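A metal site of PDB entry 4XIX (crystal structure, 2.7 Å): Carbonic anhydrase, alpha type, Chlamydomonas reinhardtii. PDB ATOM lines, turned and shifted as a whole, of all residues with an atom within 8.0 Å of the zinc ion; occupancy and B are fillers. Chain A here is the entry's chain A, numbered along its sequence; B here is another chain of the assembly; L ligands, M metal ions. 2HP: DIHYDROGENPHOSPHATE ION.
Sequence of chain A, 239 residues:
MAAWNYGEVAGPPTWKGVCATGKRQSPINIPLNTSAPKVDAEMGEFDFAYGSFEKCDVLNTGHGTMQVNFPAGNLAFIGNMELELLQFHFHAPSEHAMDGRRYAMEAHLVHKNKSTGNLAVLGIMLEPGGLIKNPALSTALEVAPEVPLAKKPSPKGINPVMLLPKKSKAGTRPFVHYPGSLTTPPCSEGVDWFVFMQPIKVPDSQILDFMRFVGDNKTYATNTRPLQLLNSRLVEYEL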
ATOM      1  N   THR A  65      -7.413   0.790   9.023  1.00  0.00           N
ATOM      2  CA  THR A  65      -8.663   0.620   8.300  1.00  0.00           C
ATOM      3  C   THR A  65      -9.065   1.836   7.523  1.00  0.00           C
ATOM      4  O   THR A  65      -8.667   2.946   7.868  1.00  0.00           O
ATOM      5  CB  THR A  65      -9.801   0.222   9.222  1.00  0.00           C
ATOM      6  OG1 THR A  65     -10.972   0.006   8.429  1.00  0.00           O
ATOM      7  CG2 THR A  65     -10.065   1.259  10.283  1.00  0.00           C
ATOM      8  N   GLN A  67     -12.537   3.947   6.294  1.00  0.00           N
ATOM      9  CA  GLN A  67     -13.787   4.210   6.981  1.00  0.00           C
ATOM     10  C   GLN A  67     -14.834   4.640   5.966  1.00  0.00           C
ATOM     11  O   GLN A  67     -14.660   5.652   5.294  1.00  0.00           O
ATOM     12  CB  GLN A  67     -13.548   5.286   8.032  1.00  0.00           C
ATOM     13  CG  GLN A  67     -14.779   5.851   8.624  1.00  0.00           C
ATOM     14  CD  GLN A  67     -14.461   6.672   9.831  1.00  0.00           C
ATOM     15  OE1 GLN A  67     -13.633   6.276  10.650  1.00  0.00           O
ATOM     16  NE2 GLN A  67     -15.115   7.823   9.964  1.00  0.00           N
ATOM     17  N   GLN A  87     -20.958   5.446  10.090  1.00  0.00           N
ATOM     18  CA  GLN A  87     -19.805   4.932   9.338  1.00  0.00           C
ATOM     19  C   GLN A  87     -19.506   3.478   9.662  1.00  0.00           C
ATOM     20  O   GLN A  87     -19.825   3.024  10.742  1.00  0.00           O
ATOM     21  CB  GLN A  87     -18.572   5.727   9.689  1.00  0.00           C
ATOM     22  CG  GLN A  87     -18.302   5.773  11.183  1.00  0.00           C
ATOM     23  CD  GLN A  87     -17.029   5.015  11.633  1.00  0.00           C
ATOM     24  OE1 GLN A  87     -16.596   4.023  11.026  1.00  0.00           O
ATOM     25  NE2 GLN A  87     -16.451   5.486  12.735  1.00  0.00           N
ATOM     26  N   PHE A  88     -18.944   2.734   8.709  1.00  0.00           N
ATOM     27  CA  PHE A  88     -18.325   1.474   9.115  1.00  0.00           C
ATOM     28  C   PHE A  88     -16.793   1.422   8.865  1.00  0.00           C
ATOM     29  O   PHE A  88     -16.252   2.233   8.118  1.00  0.00           O
ATOM     30  CB  PHE A  88     -19.073   0.277   8.555  1.00  0.00           C
ATOM     31  CG  PHE A  88     -18.939   0.079   7.092  1.00  0.00           C
ATOM     32  CD1 PHE A  88     -17.753  -0.392   6.546  1.00  0.00           C
ATOM     33  CD2 PHE A  88     -20.011   0.224   6.271  1.00  0.00           C
ATOM     34  CE1 PHE A  88     -17.644  -0.633   5.174  1.00  0.00           C
ATOM     35  CE2 PHE A  88     -19.906   0.002   4.924  1.00  0.00           C
ATOM     36  CZ  PHE A  88     -18.719  -0.432   4.378  1.00  0.00           C
ATOM     37  N   HIS A  89     -16.116   0.491   9.544  1.00  0.00           N
ATOM     38  CA  HIS A  89     -14.695   0.214   9.298  1.00  0.00           C
ATOM     39  C   HIS A  89     -14.403  -1.195   9.798  1.00  0.00           C
ATOM     40  O   HIS A  89     -15.288  -1.867  10.355  1.00  0.00           O
ATOM     41  CB  HIS A  89     -13.763   1.226   9.999  1.00  0.00           C
ATOM     42  CG  HIS A  89     -13.951   1.278  11.479  1.00  0.00           C
ATOM     43  ND1 HIS A  89     -14.857   2.121  12.076  1.00  0.00           N
ATOM     44  CD2 HIS A  89     -13.407   0.534  12.484  1.00  0.00           C
ATOM     45  CE1 HIS A  89     -14.833   1.943  13.386  1.00  0.00           C
ATOM     46  NE2 HIS A  89     -13.967   0.978  13.659  1.00  0.00           N
ATOM     47  N   PHE A  90     -13.169  -1.642   9.621  1.00  0.00           N
ATOM     48  CA  PHE A  90     -12.829  -2.996   9.946  1.00  0.00           C
ATOM     49  C   PHE A  90     -11.613  -3.076  10.819  1.00  0.00           C
ATOM     50  O   PHE A  90     -10.877  -2.095  10.980  1.00  0.00           O
ATOM     51  CB  PHE A  90     -12.599  -3.770   8.669  1.00  0.00           C
ATOM     52  CG  PHE A  90     -13.751  -3.683   7.708  1.00  0.00           C
ATOM     53  CD1 PHE A  90     -13.848  -2.604   6.829  1.00  0.00           C
ATOM     54  CD2 PHE A  90     -14.700  -4.676   7.654  1.00  0.00           C
ATOM     55  CE1 PHE A  90     -14.878  -2.529   5.924  1.00  0.00           C
ATOM     56  CE2 PHE A  90     -15.731  -4.609   6.754  1.00  0.00           C
ATOM     57  CZ  PHE A  90     -15.820  -3.532   5.875  1.00  0.00           C
ATOM     58  N   HIS A  91     -11.467  -4.241  11.445  1.00  0.00           N
ATOM     59  CA  HIS A  91     -10.347  -4.604  12.262  1.00  0.00           C
ATOM     60  C   HIS A  91      -9.996  -6.068  11.951  1.00  0.00           C
ATOM     61  O   HIS A  91     -10.901  -6.917  11.835  1.00  0.00           O
ATOM     62  CB  HIS A  91     -10.687  -4.503  13.728  1.00  0.00           C
ATOM     63  CG  HIS A  91     -10.969  -3.119  14.171  1.00  0.00           C
ATOM     64  ND1 HIS A  91      -9.992  -2.303  14.676  1.00  0.00           N
ATOM     65  CD2 HIS A  91     -12.123  -2.410  14.218  1.00  0.00           C
ATOM     66  CE1 HIS A  91     -10.517  -1.137  15.001  1.00  0.00           C
ATOM     67  NE2 HIS A  91     -11.812  -1.175  14.728  1.00  0.00           N
ATOM     68  N   GLU A  95     -11.778  -7.986  17.178  1.00  0.00           N
ATOM     69  CA  GLU A  95     -11.282  -7.336  18.398  1.00  0.00           C
ATOM     70  C   GLU A  95     -11.932  -7.984  19.577  1.00  0.00           C
ATOM     71  O   GLU A  95     -11.283  -8.278  20.557  1.00  0.00           O
ATOM     72  CB  GLU A  95     -11.558  -5.837  18.389  1.00  0.00           C
ATOM     73  CG  GLU A  95     -10.697  -5.077  17.399  1.00  0.00           C
ATOM     74  CD  GLU A  95     -10.563  -3.632  17.752  1.00  0.00           C
ATOM     75  OE1 GLU A  95     -11.527  -2.852  17.493  1.00  0.00           O
ATOM     76  OE2 GLU A  95      -9.515  -3.274  18.313  1.00  0.00           O
ATOM     77  N   HIS A  96     -13.235  -8.181  19.487  1.00  0.00           N
ATOM     78  CA  HIS A  96     -13.881  -9.024  20.452  1.00  0.00           C
ATOM     79  C   HIS A  96     -13.437 -10.457  20.176  1.00  0.00           C
ATOM     80  O   HIS A  96     -13.066 -10.795  19.054  1.00  0.00           O
ATOM     81  CB  HIS A  96     -15.401  -8.868  20.327  1.00  0.00           C
ATOM     82  CG  HIS A  96     -15.885  -7.531  20.777  1.00  0.00           C
ATOM     83  ND1 HIS A  96     -15.802  -6.406  19.992  1.00  0.00           N
ATOM     84  CD2 HIS A  96     -16.390  -7.115  21.971  1.00  0.00           C
ATOM     85  CE1 HIS A  96     -16.260  -5.360  20.666  1.00  0.00           C
ATOM     86  NE2 HIS A  96     -16.619  -5.769  21.868  1.00  0.00           N
ATOM     87  N   GLU A 106     -13.407  -8.112  11.956  1.00  0.00           N
ATOM     88  CA  GLU A 106     -14.565  -7.651  12.683  1.00  0.00           C
ATOM     89  C   GLU A 106     -14.964  -6.391  12.009  1.00  0.00           C
ATOM     90  O   GLU A 106     -14.145  -5.486  11.856  1.00  0.00           O
ATOM     91  CB  GLU A 106     -14.239  -7.352  14.153  1.00  0.00           C
ATOM     92  CG  GLU A 106     -15.439  -6.854  14.971  1.00  0.00           C
ATOM     93  CD  GLU A 106     -15.184  -6.822  16.477  1.00  0.00           C
ATOM     94  OE1 GLU A 106     -14.497  -7.719  17.026  1.00  0.00           O
ATOM     95  OE2 GLU A 106     -15.701  -5.902  17.122  1.00  0.00           O
ATOM     96  N   ALA A 107     -16.240  -6.297  11.627  1.00  0.00           N
ATOM     97  CA  ALA A 107     -16.720  -5.059  11.066  1.00  0.00           C
ATOM     98  C   ALA A 107     -17.296  -4.326  12.219  1.00  0.00           C
ATOM     99  O   ALA A 107     -17.911  -4.931  13.090  1.00  0.00           O
ATOM    100  CB  ALA A 107     -17.706  -5.326  10.044  1.00  0.00           C
ATOM    101  N   HIS A 108     -17.018  -3.031  12.269  1.00  0.00           N
ATOM    102  CA  HIS A 108     -17.680  -2.139  13.195  1.00  0.00           C
ATOM    103  C   HIS A 108     -18.592  -1.122  12.482  1.00  0.00           C
ATOM    104  O   HIS A 108     -18.095  -0.286  11.715  1.00  0.00           O
ATOM    105  CB  HIS A 108     -16.656  -1.373  13.960  1.00  0.00           C
ATOM    106  CG  HIS A 108     -16.028  -2.146  15.051  1.00  0.00           C
ATOM    107  ND1 HIS A 108     -14.837  -1.764  15.619  1.00  0.00           N
ATOM    108  CD2 HIS A 108     -16.391  -3.302  15.646  1.00  0.00           C
ATOM    109  CE1 HIS A 108     -14.493  -2.650  16.546  1.00  0.00           C
ATOM    110  NE2 HIS A 108     -15.425  -3.585  16.584  1.00  0.00           N
ATOM    111  N   LEU A 109     -19.905  -1.211  12.732  1.00  0.00           N
ATOM    112  CA  LEU A 109     -20.891  -0.229  12.209  1.00  0.00           C
ATOM    113  C   LEU A 109     -21.281   0.735  13.327  1.00  0.00           C
ATOM    114  O   LEU A 109     -22.033   0.371  14.252  1.00  0.00           O
ATOM    115  CB  LEU A 109     -22.141  -0.947  11.707  1.00  0.00           C
ATOM    116  CG  LEU A 109     -21.984  -1.650  10.374  1.00  0.00           C
ATOM    117  CD1 LEU A 109     -20.979  -2.848  10.457  1.00  0.00           C
ATOM    118  CD2 LEU A 109     -23.349  -2.089   9.827  1.00  0.00           C
ATOM    119  N   VAL A 110     -20.768   1.943  13.245  1.00  0.00           N
ATOM    120  CA  VAL A 110     -20.880   2.895  14.342  1.00  0.00           C
ATOM    121  C   VAL A 110     -22.146   3.783  14.179  1.00  0.00           C
ATOM    122  O   VAL A 110     -22.382   4.371  13.119  1.00  0.00           O
ATOM    123  CB  VAL A 110     -19.599   3.775  14.416  1.00  0.00           C
ATOM    124  CG1 VAL A 110     -19.713   4.792  15.534  1.00  0.00           C
ATOM    125  CG2 VAL A 110     -18.357   2.912  14.568  1.00  0.00           C
ATOM    126  N   VAL A 121     -22.253   0.871  18.916  1.00  0.00           N
ATOM    127  CA  VAL A 121     -21.461   0.198  17.913  1.00  0.00           C
ATOM    128  C   VAL A 121     -21.868  -1.215  17.722  1.00  0.00           C
ATOM    129  O   VAL A 121     -21.927  -1.984  18.676  1.00  0.00           O
ATOM    130  CB  VAL A 121     -19.969   0.227  18.226  1.00  0.00           C
ATOM    131  CG1 VAL A 121     -19.207  -0.376  17.054  1.00  0.00           C
ATOM    132  CG2 VAL A 121     -19.511   1.636  18.434  1.00  0.00           C
ATOM    133  N   LEU A 122     -22.145  -1.555  16.471  1.00  0.00           N
ATOM    134  CA  LEU A 122     -22.453  -2.919  16.159  1.00  0.00           C
ATOM    135  C   LEU A 122     -21.198  -3.577  15.645  1.00  0.00           C
ATOM    136  O   LEU A 122     -20.517  -3.066  14.737  1.00  0.00           O
ATOM    137  CB  LEU A 122     -23.545  -3.019  15.113  1.00  0.00           C
ATOM    138  CG  LEU A 122     -24.811  -2.194  15.299  1.00  0.00           C
ATOM    139  CD1 LEU A 122     -25.921  -2.829  14.505  1.00  0.00           C
ATOM    140  CD2 LEU A 122     -25.201  -2.052  16.749  1.00  0.00           C
ATOM    141  N   SER A 181     -16.417   1.030  25.186  1.00  0.00           N
ATOM    142  CA  SER A 181     -15.648   2.214  24.761  1.00  0.00           C
ATOM    143  C   SER A 181     -15.199   2.091  23.312  1.00  0.00           C
ATOM    144  O   SER A 181     -15.215   0.999  22.742  1.00  0.00           O
ATOM    145  CB  SER A 181     -14.399   2.345  25.629  1.00  0.00           C
ATOM    146  OG  SER A 181     -13.567   1.196  25.486  1.00  0.00           O
ATOM    147  N   LEU A 182     -14.806   3.209  22.712  1.00  0.00           N
ATOM    148  CA  LEU A 182     -14.085   3.158  21.455  1.00  0.00           C
ATOM    149  C   LEU A 182     -12.825   2.283  21.634  1.00  0.00           C
ATOM    150  O   LEU A 182     -12.189   2.293  22.690  1.00  0.00           O
ATOM    151  CB  LEU A 182     -13.677   4.567  21.052  1.00  0.00           C
ATOM    152  CG  LEU A 182     -14.841   5.481  20.735  1.00  0.00           C
ATOM    153  CD1 LEU A 182     -14.254   6.860  20.533  1.00  0.00           C
ATOM    154  CD2 LEU A 182     -15.636   4.980  19.489  1.00  0.00           C
ATOM    155  N   THR A 183     -12.461   1.508  20.618  1.00  0.00           N
ATOM    156  CA  THR A 183     -11.325   0.639  20.805  1.00  0.00           C
ATOM    157  C   THR A 183     -10.003   1.341  20.470  1.00  0.00           C
ATOM    158  O   THR A 183      -8.929   0.752  20.601  1.00  0.00           O
ATOM    159  CB  THR A 183     -11.457  -0.664  20.018  1.00  0.00           C
ATOM    160  OG1 THR A 183     -11.528  -0.363  18.628  1.00  0.00           O
ATOM    161  CG2 THR A 183     -12.687  -1.441  20.430  1.00  0.00           C
ATOM    162  N   THR A 184     -10.078   2.607  20.078  1.00  0.00           N
ATOM    163  CA  THR A 184      -8.904   3.372  19.696  1.00  0.00           C
ATOM    164  C   THR A 184      -8.910   4.668  20.465  1.00  0.00           C
ATOM    165  O   THR A 184      -9.958   5.078  20.928  1.00  0.00           O
ATOM    166  CB  THR A 184      -8.963   3.745  18.235  1.00  0.00           C
ATOM    167  OG1 THR A 184     -10.023   4.690  18.047  1.00  0.00           O
ATOM    168  CG2 THR A 184      -9.228   2.550  17.382  1.00  0.00           C
ATOM    169  N   TRP A 193     -22.314  -1.312  23.096  1.00  0.00           N
ATOM    170  CA  TRP A 193     -21.773  -2.296  22.165  1.00  0.00           C
ATOM    171  C   TRP A 193     -22.758  -3.408  21.954  1.00  0.00           C
ATOM    172  O   TRP A 193     -23.223  -4.034  22.918  1.00  0.00           O
ATOM    173  CB  TRP A 193     -20.436  -2.911  22.706  1.00  0.00           C
ATOM    174  CG  TRP A 193     -19.269  -2.136  22.354  1.00  0.00           C
ATOM    175  CD1 TRP A 193     -18.663  -1.197  23.112  1.00  0.00           C
ATOM    176  CD2 TRP A 193     -18.589  -2.146  21.102  1.00  0.00           C
ATOM    177  NE1 TRP A 193     -17.633  -0.636  22.418  1.00  0.00           N
ATOM    178  CE2 TRP A 193     -17.573  -1.209  21.178  1.00  0.00           C
ATOM    179  CE3 TRP A 193     -18.747  -2.888  19.936  1.00  0.00           C
ATOM    180  CZ2 TRP A 193     -16.705  -0.980  20.124  1.00  0.00           C
ATOM    181  CZ3 TRP A 193     -17.887  -2.651  18.891  1.00  0.00           C
ATOM    182  CH2 TRP A 193     -16.871  -1.711  18.989  1.00  0.00           C
ATOM    183  N   ASN A 223      -4.684  -4.495  13.065  1.00  0.00           N
ATOM    184  CA  ASN A 223      -5.108  -3.233  13.670  1.00  0.00           C
ATOM    185  C   ASN A 223      -6.175  -3.430  14.717  1.00  0.00           C
ATOM    186  O   ASN A 223      -7.265  -2.823  14.661  1.00  0.00           O
ATOM    187  CB  ASN A 223      -5.584  -2.233  12.613  1.00  0.00           C
ATOM    188  CG  ASN A 223      -6.885  -2.636  11.984  1.00  0.00           C
ATOM    189  OD1 ASN A 223      -7.151  -3.823  11.805  1.00  0.00           O
ATOM    190  ND2 ASN A 223      -7.708  -1.634  11.656  1.00  0.00           N
ATOM    191  N   TYR B   6      -0.716   1.280  16.132  1.00  0.00           N
ATOM    192  CA  TYR B   6      -0.616  -0.073  16.609  1.00  0.00           C
ATOM    193  C   TYR B   6       0.822  -0.601  16.718  1.00  0.00           C
ATOM    194  O   TYR B   6       1.210  -1.273  17.648  1.00  0.00           O
ATOM    195  CB  TYR B   6      -1.412  -0.950  15.692  1.00  0.00           C
ATOM    196  CG  TYR B   6      -2.866  -0.678  15.768  1.00  0.00           C
ATOM    197  CD1 TYR B   6      -3.607  -1.214  16.738  1.00  0.00           C
ATOM    198  CD2 TYR B   6      -3.450   0.143  14.877  1.00  0.00           C
ATOM    199  CE1 TYR B   6      -4.904  -0.940  16.832  1.00  0.00           C
ATOM    200  CE2 TYR B   6      -4.752   0.433  14.974  1.00  0.00           C
ATOM    201  CZ  TYR B   6      -5.489  -0.124  15.933  1.00  0.00           C
ATOM    202  OH  TYR B   6      -6.802   0.129  15.971  1.00  0.00           O
HETATM  203  P   2HP L   1     -13.501   2.036  17.086  1.00  0.00           P
HETATM  204  O1  2HP L   1     -14.874   2.567  16.569  1.00  0.00           O
HETATM  205  O2  2HP L   1     -13.082   2.846  18.340  1.00  0.00           O
HETATM  206  O3  2HP L   1     -12.427   2.187  15.971  1.00  0.00           O
HETATM  207  O4  2HP L   1     -13.646   0.530  17.464  1.00  0.00           O
HETATM  208 ZN    ZN M   1     -13.537  -0.204  15.290  1.00  0.00          ZN
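The zinc ion is bound by a ring nitrogen (NE2) of His 91, a ring nitrogen (ND1) of His 108, a ring nitrogen (NE2) of His 89 and an oxygen (O4) of the ligand. The zinc ion has four donor atoms within binding distance. Slightly farther from the zinc ion lies an oxygen (O3) of the ligand (2.7 Å).
Glu 95 touches the zinc ion (OE1 to ZN, 3.99 Å). Thr 183 touches the zinc ion (OG1 to ZN, 3.9 Å). Of the 23 residues printed, 5 come within 4 Å of the zinc ion. The nearest printed residue that does not touch the zinc ion is Trp 193 (5.2 Å).
OE1 of Glu 95 lies close to ND1 of His 91, at 3.3 Å. The backbone carbonyl oxygen (O) of His 91 is in hydrogen-bond range of the backbone NH (N) of Glu 106 (2.8 Å). A ring nitrogen (ND1) of His 91 is in hydrogen-bond range of the backbone carbonyl oxygen of Asn 223, 2.8 Å away. ND1 of His 89 lies within hydrogen-bond range of OE1 of Gln 87. OE1 of Glu 95 sits at hydrogen-bond distance from OG1 of Thr 183 (2.7 Å). N of Glu 95 sits at hydrogen-bond distance from OE1 of Glu 106 (2.7 Å).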
